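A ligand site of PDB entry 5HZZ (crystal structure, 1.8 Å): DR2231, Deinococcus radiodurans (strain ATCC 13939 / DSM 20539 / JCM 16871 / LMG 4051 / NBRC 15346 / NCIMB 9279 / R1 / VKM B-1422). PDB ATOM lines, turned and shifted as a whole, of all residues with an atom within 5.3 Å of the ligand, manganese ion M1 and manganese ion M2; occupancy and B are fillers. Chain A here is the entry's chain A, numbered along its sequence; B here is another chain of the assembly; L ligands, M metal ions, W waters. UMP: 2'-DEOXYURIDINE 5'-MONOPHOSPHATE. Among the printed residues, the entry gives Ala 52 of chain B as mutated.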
ATOM      1  N   VAL A 110      -3.451  12.129  20.946  1.00  0.00           N
ATOM      2  CA  VAL A 110      -4.545  12.741  20.190  1.00  0.00           C
ATOM      3  C   VAL A 110      -3.994  13.730  19.167  1.00  0.00           C
ATOM      4  O   VAL A 110      -4.445  13.782  18.019  1.00  0.00           O
ATOM      5  CB  VAL A 110      -5.530  13.401  21.163  1.00  0.00           C
ATOM      6  CG1 VAL A 110      -6.508  14.324  20.428  1.00  0.00           C
ATOM      7  CG2 VAL A 110      -6.328  12.314  21.904  1.00  0.00           C
ATOM      8  N   ASN A 114      -4.236  13.994  15.015  1.00  0.00           N
ATOM      9  CA  ASN A 114      -4.889  15.135  14.374  1.00  0.00           C
ATOM     10  C   ASN A 114      -4.013  15.740  13.281  1.00  0.00           C
ATOM     11  O   ASN A 114      -4.533  16.078  12.219  1.00  0.00           O
ATOM     12  CB  ASN A 114      -5.283  16.183  15.429  1.00  0.00           C
ATOM     13  CG  ASN A 114      -6.531  15.754  16.200  1.00  0.00           C
ATOM     14  OD1 ASN A 114      -7.296  14.901  15.725  1.00  0.00           O
ATOM     15  ND2 ASN A 114      -6.754  16.335  17.378  1.00  0.00           N
ATOM     16  N   LYS A 117      -4.456  14.290   9.853  1.00  0.00           N
ATOM     17  CA  LYS A 117      -5.618  14.631   9.048  1.00  0.00           C
ATOM     18  C   LYS A 117      -5.334  15.687   7.995  1.00  0.00           C
ATOM     19  O   LYS A 117      -6.233  15.997   7.217  1.00  0.00           O
ATOM     20  CB  LYS A 117      -6.767  15.123   9.919  1.00  0.00           C
ATOM     21  CG  LYS A 117      -7.183  14.114  11.002  1.00  0.00           C
ATOM     22  CD  LYS A 117      -8.137  14.757  12.015  1.00  0.00           C
ATOM     23  CE  LYS A 117      -8.609  13.739  13.063  1.00  0.00           C
ATOM     24  NZ  LYS A 117      -9.597  14.386  14.018  1.00  0.00           N
ATOM     25  N   GLY A 126     -15.707  24.637   7.995  1.00  0.00           N
ATOM     26  CA  GLY A 126     -14.285  24.742   8.259  1.00  0.00           C
ATOM     27  C   GLY A 126     -13.714  23.570   9.016  1.00  0.00           C
ATOM     28  O   GLY A 126     -12.480  23.505   9.183  1.00  0.00           O
ATOM     29  N   LYS A 127     -14.553  22.637   9.465  1.00  0.00           N
ATOM     30  CA  LYS A 127     -14.034  21.514  10.234  1.00  0.00           C
ATOM     31  C   LYS A 127     -13.117  20.660   9.371  1.00  0.00           C
ATOM     32  O   LYS A 127     -13.464  20.313   8.237  1.00  0.00           O
ATOM     33  CB  LYS A 127     -15.160  20.649  10.786  1.00  0.00           C
ATOM     34  CG  LYS A 127     -14.610  19.518  11.643  1.00  0.00           C
ATOM     35  CD  LYS A 127     -15.724  18.637  12.248  1.00  0.00           C
ATOM     36  CE  LYS A 127     -15.122  17.616  13.224  1.00  0.00           C
ATOM     37  NZ  LYS A 127     -16.178  16.702  13.805  1.00  0.00           N
ATOM     38  N   GLN A 128     -11.935  20.356   9.902  1.00  0.00           N
ATOM     39  CA  GLN A 128     -11.007  19.462   9.213  1.00  0.00           C
ATOM     40  C   GLN A 128     -11.533  18.043   9.292  1.00  0.00           C
ATOM     41  O   GLN A 128     -11.878  17.557  10.371  1.00  0.00           O
ATOM     42  CB  GLN A 128      -9.622  19.536   9.855  1.00  0.00           C
ATOM     43  CG  GLN A 128      -8.613  18.584   9.205  1.00  0.00           C
ATOM     44  CD  GLN A 128      -8.384  18.916   7.730  1.00  0.00           C
ATOM     45  OE1 GLN A 128      -8.027  20.040   7.391  1.00  0.00           O
ATOM     46  NE2 GLN A 128      -8.624  17.945   6.847  1.00  0.00           N
ATOM     47  N   LYS A 130     -11.286  13.760   7.959  1.00  0.00           N
ATOM     48  CA  LYS A 130     -10.252  12.714   7.956  1.00  0.00           C
ATOM     49  C   LYS A 130      -9.990  12.246   6.530  1.00  0.00           C
ATOM     50  O   LYS A 130     -10.938  11.992   5.777  1.00  0.00           O
ATOM     51  CB  LYS A 130     -10.690  11.548   8.816  1.00  0.00           C
ATOM     52  CG  LYS A 130     -10.754  11.914  10.302  1.00  0.00           C
ATOM     53  CD  LYS A 130     -11.821  11.092  11.057  1.00  0.00           C
ATOM     54  CE  LYS A 130     -11.871  11.526  12.536  1.00  0.00           C
ATOM     55  NZ  LYS A 130     -13.031  10.930  13.252  1.00  0.00           N
ATOM     56  N   LEU B  19      -1.502  23.177  19.262  1.00  0.00           N
ATOM     57  CA  LEU B  19      -2.624  23.637  18.445  1.00  0.00           C
ATOM     58  C   LEU B  19      -2.157  24.551  17.322  1.00  0.00           C
ATOM     59  O   LEU B  19      -2.668  24.485  16.197  1.00  0.00           O
ATOM     60  CB  LEU B  19      -3.677  24.340  19.311  1.00  0.00           C
ATOM     61  CG  LEU B  19      -4.911  23.478  19.564  1.00  0.00           C
ATOM     62  CD1 LEU B  19      -5.637  23.156  18.247  1.00  0.00           C
ATOM     63  CD2 LEU B  19      -4.562  22.156  20.290  1.00  0.00           C
ATOM     64  N   PHE B  22      -0.899  22.361  14.604  1.00  0.00           N
ATOM     65  CA  PHE B  22      -2.011  21.742  13.879  1.00  0.00           C
ATOM     66  C   PHE B  22      -2.674  22.724  12.929  1.00  0.00           C
ATOM     67  O   PHE B  22      -2.917  22.417  11.752  1.00  0.00           O
ATOM     68  CB  PHE B  22      -3.010  21.185  14.902  1.00  0.00           C
ATOM     69  CG  PHE B  22      -4.293  20.692  14.300  1.00  0.00           C
ATOM     70  CD1 PHE B  22      -4.335  19.536  13.535  1.00  0.00           C
ATOM     71  CD2 PHE B  22      -5.477  21.391  14.552  1.00  0.00           C
ATOM     72  CE1 PHE B  22      -5.551  19.081  13.012  1.00  0.00           C
ATOM     73  CE2 PHE B  22      -6.695  20.945  14.041  1.00  0.00           C
ATOM     74  CZ  PHE B  22      -6.732  19.788  13.258  1.00  0.00           C
ATOM     75  N   HIS B  23      -2.969  23.928  13.402  1.00  0.00           N
ATOM     76  CA  HIS B  23      -3.660  24.889  12.535  1.00  0.00           C
ATOM     77  C   HIS B  23      -2.770  25.319  11.364  1.00  0.00           C
ATOM     78  O   HIS B  23      -3.270  25.515  10.254  1.00  0.00           O
ATOM     79  CB  HIS B  23      -4.144  26.072  13.356  1.00  0.00           C
ATOM     80  CG  HIS B  23      -5.369  25.757  14.171  1.00  0.00           C
ATOM     81  ND1 HIS B  23      -5.691  26.402  15.346  1.00  0.00           N
ATOM     82  CD2 HIS B  23      -6.338  24.836  13.958  1.00  0.00           C
ATOM     83  CE1 HIS B  23      -6.805  25.879  15.831  1.00  0.00           C
ATOM     84  NE2 HIS B  23      -7.224  24.939  15.007  1.00  0.00           N
ATOM     85  N   ILE B  26      -3.001  22.482   8.781  1.00  0.00           N
ATOM     86  CA  ILE B  26      -4.233  22.309   8.029  1.00  0.00           C
ATOM     87  C   ILE B  26      -4.651  23.574   7.302  1.00  0.00           C
ATOM     88  O   ILE B  26      -5.683  23.577   6.607  1.00  0.00           O
ATOM     89  CB  ILE B  26      -5.384  21.808   8.929  1.00  0.00           C
ATOM     90  CG1 ILE B  26      -5.824  22.902   9.926  1.00  0.00           C
ATOM     91  CG2 ILE B  26      -4.972  20.514   9.650  1.00  0.00           C
ATOM     92  CD1 ILE B  26      -7.165  22.584  10.585  1.00  0.00           C
ATOM     93  N   LEU B  44     -17.864  28.044  14.101  1.00  0.00           N
ATOM     94  CA  LEU B  44     -17.161  26.771  14.093  1.00  0.00           C
ATOM     95  C   LEU B  44     -16.668  26.395  15.476  1.00  0.00           C
ATOM     96  O   LEU B  44     -16.768  25.239  15.889  1.00  0.00           O
ATOM     97  CB  LEU B  44     -15.974  26.810  13.130  1.00  0.00           C
ATOM     98  CG  LEU B  44     -15.090  25.551  13.212  1.00  0.00           C
ATOM     99  CD1 LEU B  44     -15.861  24.350  12.711  1.00  0.00           C
ATOM    100  CD2 LEU B  44     -13.802  25.750  12.386  1.00  0.00           C
ATOM    101  N   ARG B  45     -16.067  27.344  16.192  1.00  0.00           N
ATOM    102  CA  ARG B  45     -15.547  27.010  17.521  1.00  0.00           C
ATOM    103  C   ARG B  45     -16.670  26.532  18.429  1.00  0.00           C
ATOM    104  O   ARG B  45     -16.492  25.575  19.207  1.00  0.00           O
ATOM    105  CB  ARG B  45     -14.826  28.198  18.159  1.00  0.00           C
ATOM    106  CG  ARG B  45     -13.609  28.796  17.400  1.00  0.00           C
ATOM    107  CD  ARG B  45     -12.681  27.775  16.712  1.00  0.00           C
ATOM    108  NE  ARG B  45     -12.247  26.660  17.563  1.00  0.00           N
ATOM    109  CZ  ARG B  45     -11.450  25.688  17.116  1.00  0.00           C
ATOM    110  NH1 ARG B  45     -10.983  25.739  15.872  1.00  0.00           N
ATOM    111  NH2 ARG B  45     -11.119  24.664  17.913  1.00  0.00           N
ATOM    112  N   LEU B  48     -17.557  22.885  17.438  1.00  0.00           N
ATOM    113  CA  LEU B  48     -16.590  21.898  17.908  1.00  0.00           C
ATOM    114  C   LEU B  48     -16.674  21.721  19.425  1.00  0.00           C
ATOM    115  O   LEU B  48     -16.499  20.610  19.938  1.00  0.00           O
ATOM    116  CB  LEU B  48     -15.176  22.320  17.489  1.00  0.00           C
ATOM    117  CG  LEU B  48     -14.955  22.418  15.969  1.00  0.00           C
ATOM    118  CD1 LEU B  48     -13.570  22.997  15.649  1.00  0.00           C
ATOM    119  CD2 LEU B  48     -15.158  21.029  15.293  1.00  0.00           C
ATOM    120  N   GLU B  51     -19.791  19.681  20.148  1.00  0.00           N
ATOM    121  CA  GLU B  51     -19.597  18.293  19.750  1.00  0.00           C
ATOM    122  C   GLU B  51     -18.709  17.543  20.739  1.00  0.00           C
ATOM    123  O   GLU B  51     -19.001  16.411  21.129  1.00  0.00           O
ATOM    124  CB  GLU B  51     -18.984  18.223  18.345  1.00  0.00           C
ATOM    125  CG  GLU B  51     -18.632  16.815  17.911  1.00  0.00           C
ATOM    126  CD  GLU B  51     -17.966  16.747  16.546  1.00  0.00           C
ATOM    127  OE1 GLU B  51     -17.762  17.820  15.903  1.00  0.00           O
ATOM    128  OE2 GLU B  51     -17.640  15.616  16.133  1.00  0.00           O
ATOM    129  N   ALA B  52     -17.609  18.179  21.169  1.00  0.00           N
ATOM    130  CA  ALA B  52     -16.686  17.519  22.087  1.00  0.00           C
ATOM    131  C   ALA B  52     -17.318  17.310  23.451  1.00  0.00           C
ATOM    132  O   ALA B  52     -17.137  16.255  24.078  1.00  0.00           O
ATOM    133  CB  ALA B  52     -15.386  18.316  22.207  1.00  0.00           C
ATOM    134  N   GLU B  55     -19.649  14.346  23.389  1.00  0.00           N
ATOM    135  CA  GLU B  55     -18.925  13.084  23.388  1.00  0.00           C
ATOM    136  C   GLU B  55     -18.413  12.727  24.787  1.00  0.00           C
ATOM    137  O   GLU B  55     -18.455  11.562  25.176  1.00  0.00           O
ATOM    138  CB  GLU B  55     -17.749  13.131  22.414  1.00  0.00           C
ATOM    139  CG  GLU B  55     -18.152  13.072  20.941  1.00  0.00           C
ATOM    140  CD  GLU B  55     -17.158  13.768  20.037  1.00  0.00           C
ATOM    141  OE1 GLU B  55     -16.125  14.284  20.538  1.00  0.00           O
ATOM    142  OE2 GLU B  55     -17.413  13.805  18.822  1.00  0.00           O
ATOM    143  N   GLU B  84     -11.917  11.451  24.929  1.00  0.00           N
ATOM    144  CA  GLU B  84     -12.854  12.537  24.693  1.00  0.00           C
ATOM    145  C   GLU B  84     -12.521  13.769  25.519  1.00  0.00           C
ATOM    146  O   GLU B  84     -12.740  14.901  25.053  1.00  0.00           O
ATOM    147  CB  GLU B  84     -14.288  12.083  24.956  1.00  0.00           C
ATOM    148  CG  GLU B  84     -14.718  10.881  24.117  1.00  0.00           C
ATOM    149  CD  GLU B  84     -14.712  11.133  22.602  1.00  0.00           C
ATOM    150  OE1 GLU B  84     -14.650  12.295  22.147  1.00  0.00           O
ATOM    151  OE2 GLU B  84     -14.784  10.135  21.868  1.00  0.00           O
ATOM    152  N   ALA B  86      -9.491  14.676  26.203  1.00  0.00           N
ATOM    153  CA  ALA B  86      -8.376  15.254  25.462  1.00  0.00           C
ATOM    154  C   ALA B  86      -8.852  15.988  24.212  1.00  0.00           C
ATOM    155  O   ALA B  86      -8.318  17.043  23.864  1.00  0.00           O
ATOM    156  CB  ALA B  86      -7.361  14.170  25.105  1.00  0.00           C
ATOM    157  N   ASP B  87      -9.880  15.451  23.545  1.00  0.00           N
ATOM    158  CA  ASP B  87     -10.526  16.173  22.438  1.00  0.00           C
ATOM    159  C   ASP B  87     -11.122  17.496  22.904  1.00  0.00           C
ATOM    160  O   ASP B  87     -11.078  18.497  22.186  1.00  0.00           O
ATOM    161  CB  ASP B  87     -11.634  15.332  21.828  1.00  0.00           C
ATOM    162  CG  ASP B  87     -11.148  14.292  20.836  1.00  0.00           C
ATOM    163  OD1 ASP B  87      -9.956  14.305  20.431  1.00  0.00           O
ATOM    164  OD2 ASP B  87     -11.987  13.455  20.459  1.00  0.00           O
ATOM    165  N   TYR B  90      -8.468  19.820  23.259  1.00  0.00           N
ATOM    166  CA  TYR B  90      -7.959  20.186  21.940  1.00  0.00           C
ATOM    167  C   TYR B  90      -8.758  21.317  21.315  1.00  0.00           C
ATOM    168  O   TYR B  90      -8.184  22.286  20.795  1.00  0.00           O
ATOM    169  CB  TYR B  90      -7.953  18.949  21.048  1.00  0.00           C
ATOM    170  CG  TYR B  90      -6.833  18.981  20.015  1.00  0.00           C
ATOM    171  CD1 TYR B  90      -7.015  19.602  18.776  1.00  0.00           C
ATOM    172  CD2 TYR B  90      -5.600  18.388  20.275  1.00  0.00           C
ATOM    173  CE1 TYR B  90      -5.985  19.627  17.837  1.00  0.00           C
ATOM    174  CE2 TYR B  90      -4.567  18.425  19.354  1.00  0.00           C
ATOM    175  CZ  TYR B  90      -4.775  19.036  18.125  1.00  0.00           C
ATOM    176  OH  TYR B  90      -3.761  19.070  17.194  1.00  0.00           O
ATOM    177  N   VAL B  91     -10.094  21.235  21.378  1.00  0.00           N
ATOM    178  CA  VAL B  91     -10.898  22.292  20.755  1.00  0.00           C
ATOM    179  C   VAL B  91     -11.007  23.540  21.621  1.00  0.00           C
ATOM    180  O   VAL B  91     -11.344  24.613  21.097  1.00  0.00           O
ATOM    181  CB  VAL B  91     -12.302  21.793  20.377  1.00  0.00           C
ATOM    182  CG1 VAL B  91     -12.209  20.657  19.343  1.00  0.00           C
ATOM    183  CG2 VAL B  91     -13.113  21.384  21.588  1.00  0.00           C
HETATM  184  N1  UMP L   1     -10.187  18.719  15.371  1.00  0.00           N
HETATM  185  C2  UMP L   1      -9.899  20.164  15.515  1.00  0.00           C
HETATM  186  N3  UMP L   1     -10.350  21.094  14.438  1.00  0.00           N
HETATM  187  C4  UMP L   1     -11.076  20.585  13.300  1.00  0.00           C
HETATM  188  C5  UMP L   1     -11.366  19.136  13.186  1.00  0.00           C
HETATM  189  C6  UMP L   1     -10.913  18.209  14.233  1.00  0.00           C
HETATM  190  O2  UMP L   1      -9.312  20.572  16.459  1.00  0.00           O
HETATM  191  O4  UMP L   1     -11.439  21.348  12.463  1.00  0.00           O
HETATM  192  C1' UMP L   1      -9.714  17.803  16.424  1.00  0.00           C
HETATM  193  C2' UMP L   1     -10.494  18.005  17.772  1.00  0.00           C
HETATM  194  C3' UMP L   1     -10.638  16.562  18.246  1.00  0.00           C
HETATM  195  C4' UMP L   1     -10.795  15.821  17.117  1.00  0.00           C
HETATM  196  O3' UMP L   1      -9.386  16.197  18.947  1.00  0.00           O
HETATM  197  O4' UMP L   1      -9.931  16.573  15.996  1.00  0.00           O
HETATM  198  C5' UMP L   1     -12.207  15.815  16.646  1.00  0.00           C
HETATM  199  O5' UMP L   1     -12.278  15.292  15.327  1.00  0.00           O
HETATM  200  P   UMP L   1     -13.540  14.316  14.925  1.00  0.00           P
HETATM  201  OP1 UMP L   1     -13.610  14.270  13.407  1.00  0.00           O
HETATM  202  OP2 UMP L   1     -14.820  14.911  15.448  1.00  0.00           O
HETATM  203  OP3 UMP L   1     -13.285  12.948  15.516  1.00  0.00           O
HETATM  204 MN    MN M   1     -16.084  14.367  17.187  1.00  0.00          MN
HETATM  205 MN    MN M   2     -14.145  13.920  20.342  1.00  0.00          MN
HETATM  206  O   HOH W   1     -16.873  12.716  16.079  1.00  0.00           O
HETATM  207  O   HOH W   2     -14.670  15.097  23.054  1.00  0.00           O
HETATM  208  O   HOH W   3     -11.585  15.346  12.261  1.00  0.00           O
HETATM  209  O   HOH W   4     -15.067  13.393  11.394  1.00  0.00           O
HETATM  210  O   HOH W   5     -10.206  24.090  11.689  1.00  0.00           O
HETATM  211  O   HOH W   6      -9.617  23.768  14.366  1.00  0.00           O
HETATM  212  O   HOH W   7     -10.607  12.454  15.745  1.00  0.00           O
HETATM  213  O   HOH W   8     -12.465  11.266  19.171  1.00  0.00           O
HETATM  214  O   HOH W   9      -8.928  23.001  17.326  1.00  0.00           O
HETATM  215  O   HOH W  10     -14.730  12.943  17.904  1.00  0.00           O
HETATM  216  O   HOH W  11     -15.047  16.134  18.672  1.00  0.00           O
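N of Gln 128 sits at hydrogen-bond distance from O4 of the ligand (2.8 Å).
OD1 of Asp 87 of chain B is in hydrogen-bond range of O3' of the ligand.
An oxygen (O3') of the ligand sits at hydrogen-bond distance from the side-chain amide nitrogen (ND2) of Asn 114, 3.1 Å away.
OP1 of the ligand is in salt-bridge range of NZ of Lys 127 (3.6 Å).
An oxygen (O4') of the ligand sits at hydrogen-bond distance from the side-chain amino group (NZ) of Lys 117.
An oxygen (OP3) of the ligand lies within salt-bridge range of the side-chain amino group of Lys 130, at 3.0 Å.
The backbone carbonyl oxygen (O) of Val 91 of chain B is in hydrogen-bond range of the guanidinium group (NH2) of Arg 45 of chain B, 3.2 Å away.
The side-chain amino group (NZ) of Lys 117 is in hydrogen-bond range of the side-chain amide oxygen (OD1) of Asn 114 (2.9 Å).
OE1 of Glu 51 of chain B is in salt-bridge range of NZ of Lys 127.
The side-chain amide nitrogen of Gln 128 lies within hydrogen-bond range of the backbone carbonyl oxygen of Lys 117 (3.1 Å).
Val 110 touches the ligand.
CE2 of Phe 22 of chain B touches O2 of the ligand, 3.6 Å away.
CD1 of Leu 48 of chain B touches N3 of the ligand, 3.9 Å away.
CD1 of Tyr 90 of chain B touches O2 of the ligand, 3.4 Å away.
Val 91 of chain B touches the ligand (CG1 to C2', 3.5 Å).
The nearest printed residue that does not touch the ligand is Gly 126 (4.1 Å).
Three residues have an atom within 4 Å of manganese ion M2: Glu 55 of chain B, Glu 84 of chain B and Asp 87 of chain B.
Manganese ion M1 is bound by water W10 (2.1 Å), water W1 (2.1 Å), the side-chain carboxylate of Glu 55 of chain B (2.2 Å), an oxygen (OP2) of the ligand (2.2 Å), the side-chain carboxylate of Glu 51 of chain B (2.3 Å) and water W11 (2.5 Å).
Manganese ion M1 has six donor atoms within binding distance.
Manganese ion M2 is bound by OE1 of Glu 55 of chain B (2.0 Å), OD2 of Asp 87 of chain B (2.2 Å), OE1 of Glu 84 of chain B (2.5 Å) and water W10 (2.7 Å).
Manganese ion M2 has four donor atoms within binding distance.
Slightly farther from manganese ion M2 lies water W11 (2.9 Å).
Water W3 lies within hydrogen-bond range of OP1 of the ligand (2.6 Å), NZ of Lys 117 (2.8 Å) and O of Gln 128 (2.9 Å).
Water W9 lies within hydrogen-bond range of an oxygen (O2) of the ligand (2.6 Å), the guanidinium group of Arg 45 of chain B (2.8 Å) and a ring nitrogen (NE2) of His 23 of chain B (3.5 Å).
Water W7 bridges an oxygen (OP3) of the ligand (2.7 Å) and the side-chain amino group (NZ) of Lys 117 (2.8 Å).
Water W6 lies within hydrogen-bond range of NE2 of His 23 of chain B (2.7 Å), N3 of the ligand (2.8 Å) and NH1 of Arg 45 of chain B (2.8 Å).
Water W2 lies within hydrogen-bond range of the backbone carbonyl oxygen of Glu 84 of chain B (2.8 Å) and the backbone carbonyl oxygen of Ala 52 of chain B (2.9 Å).
Water W5 bridges O4 of the ligand and O of Gly 126.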
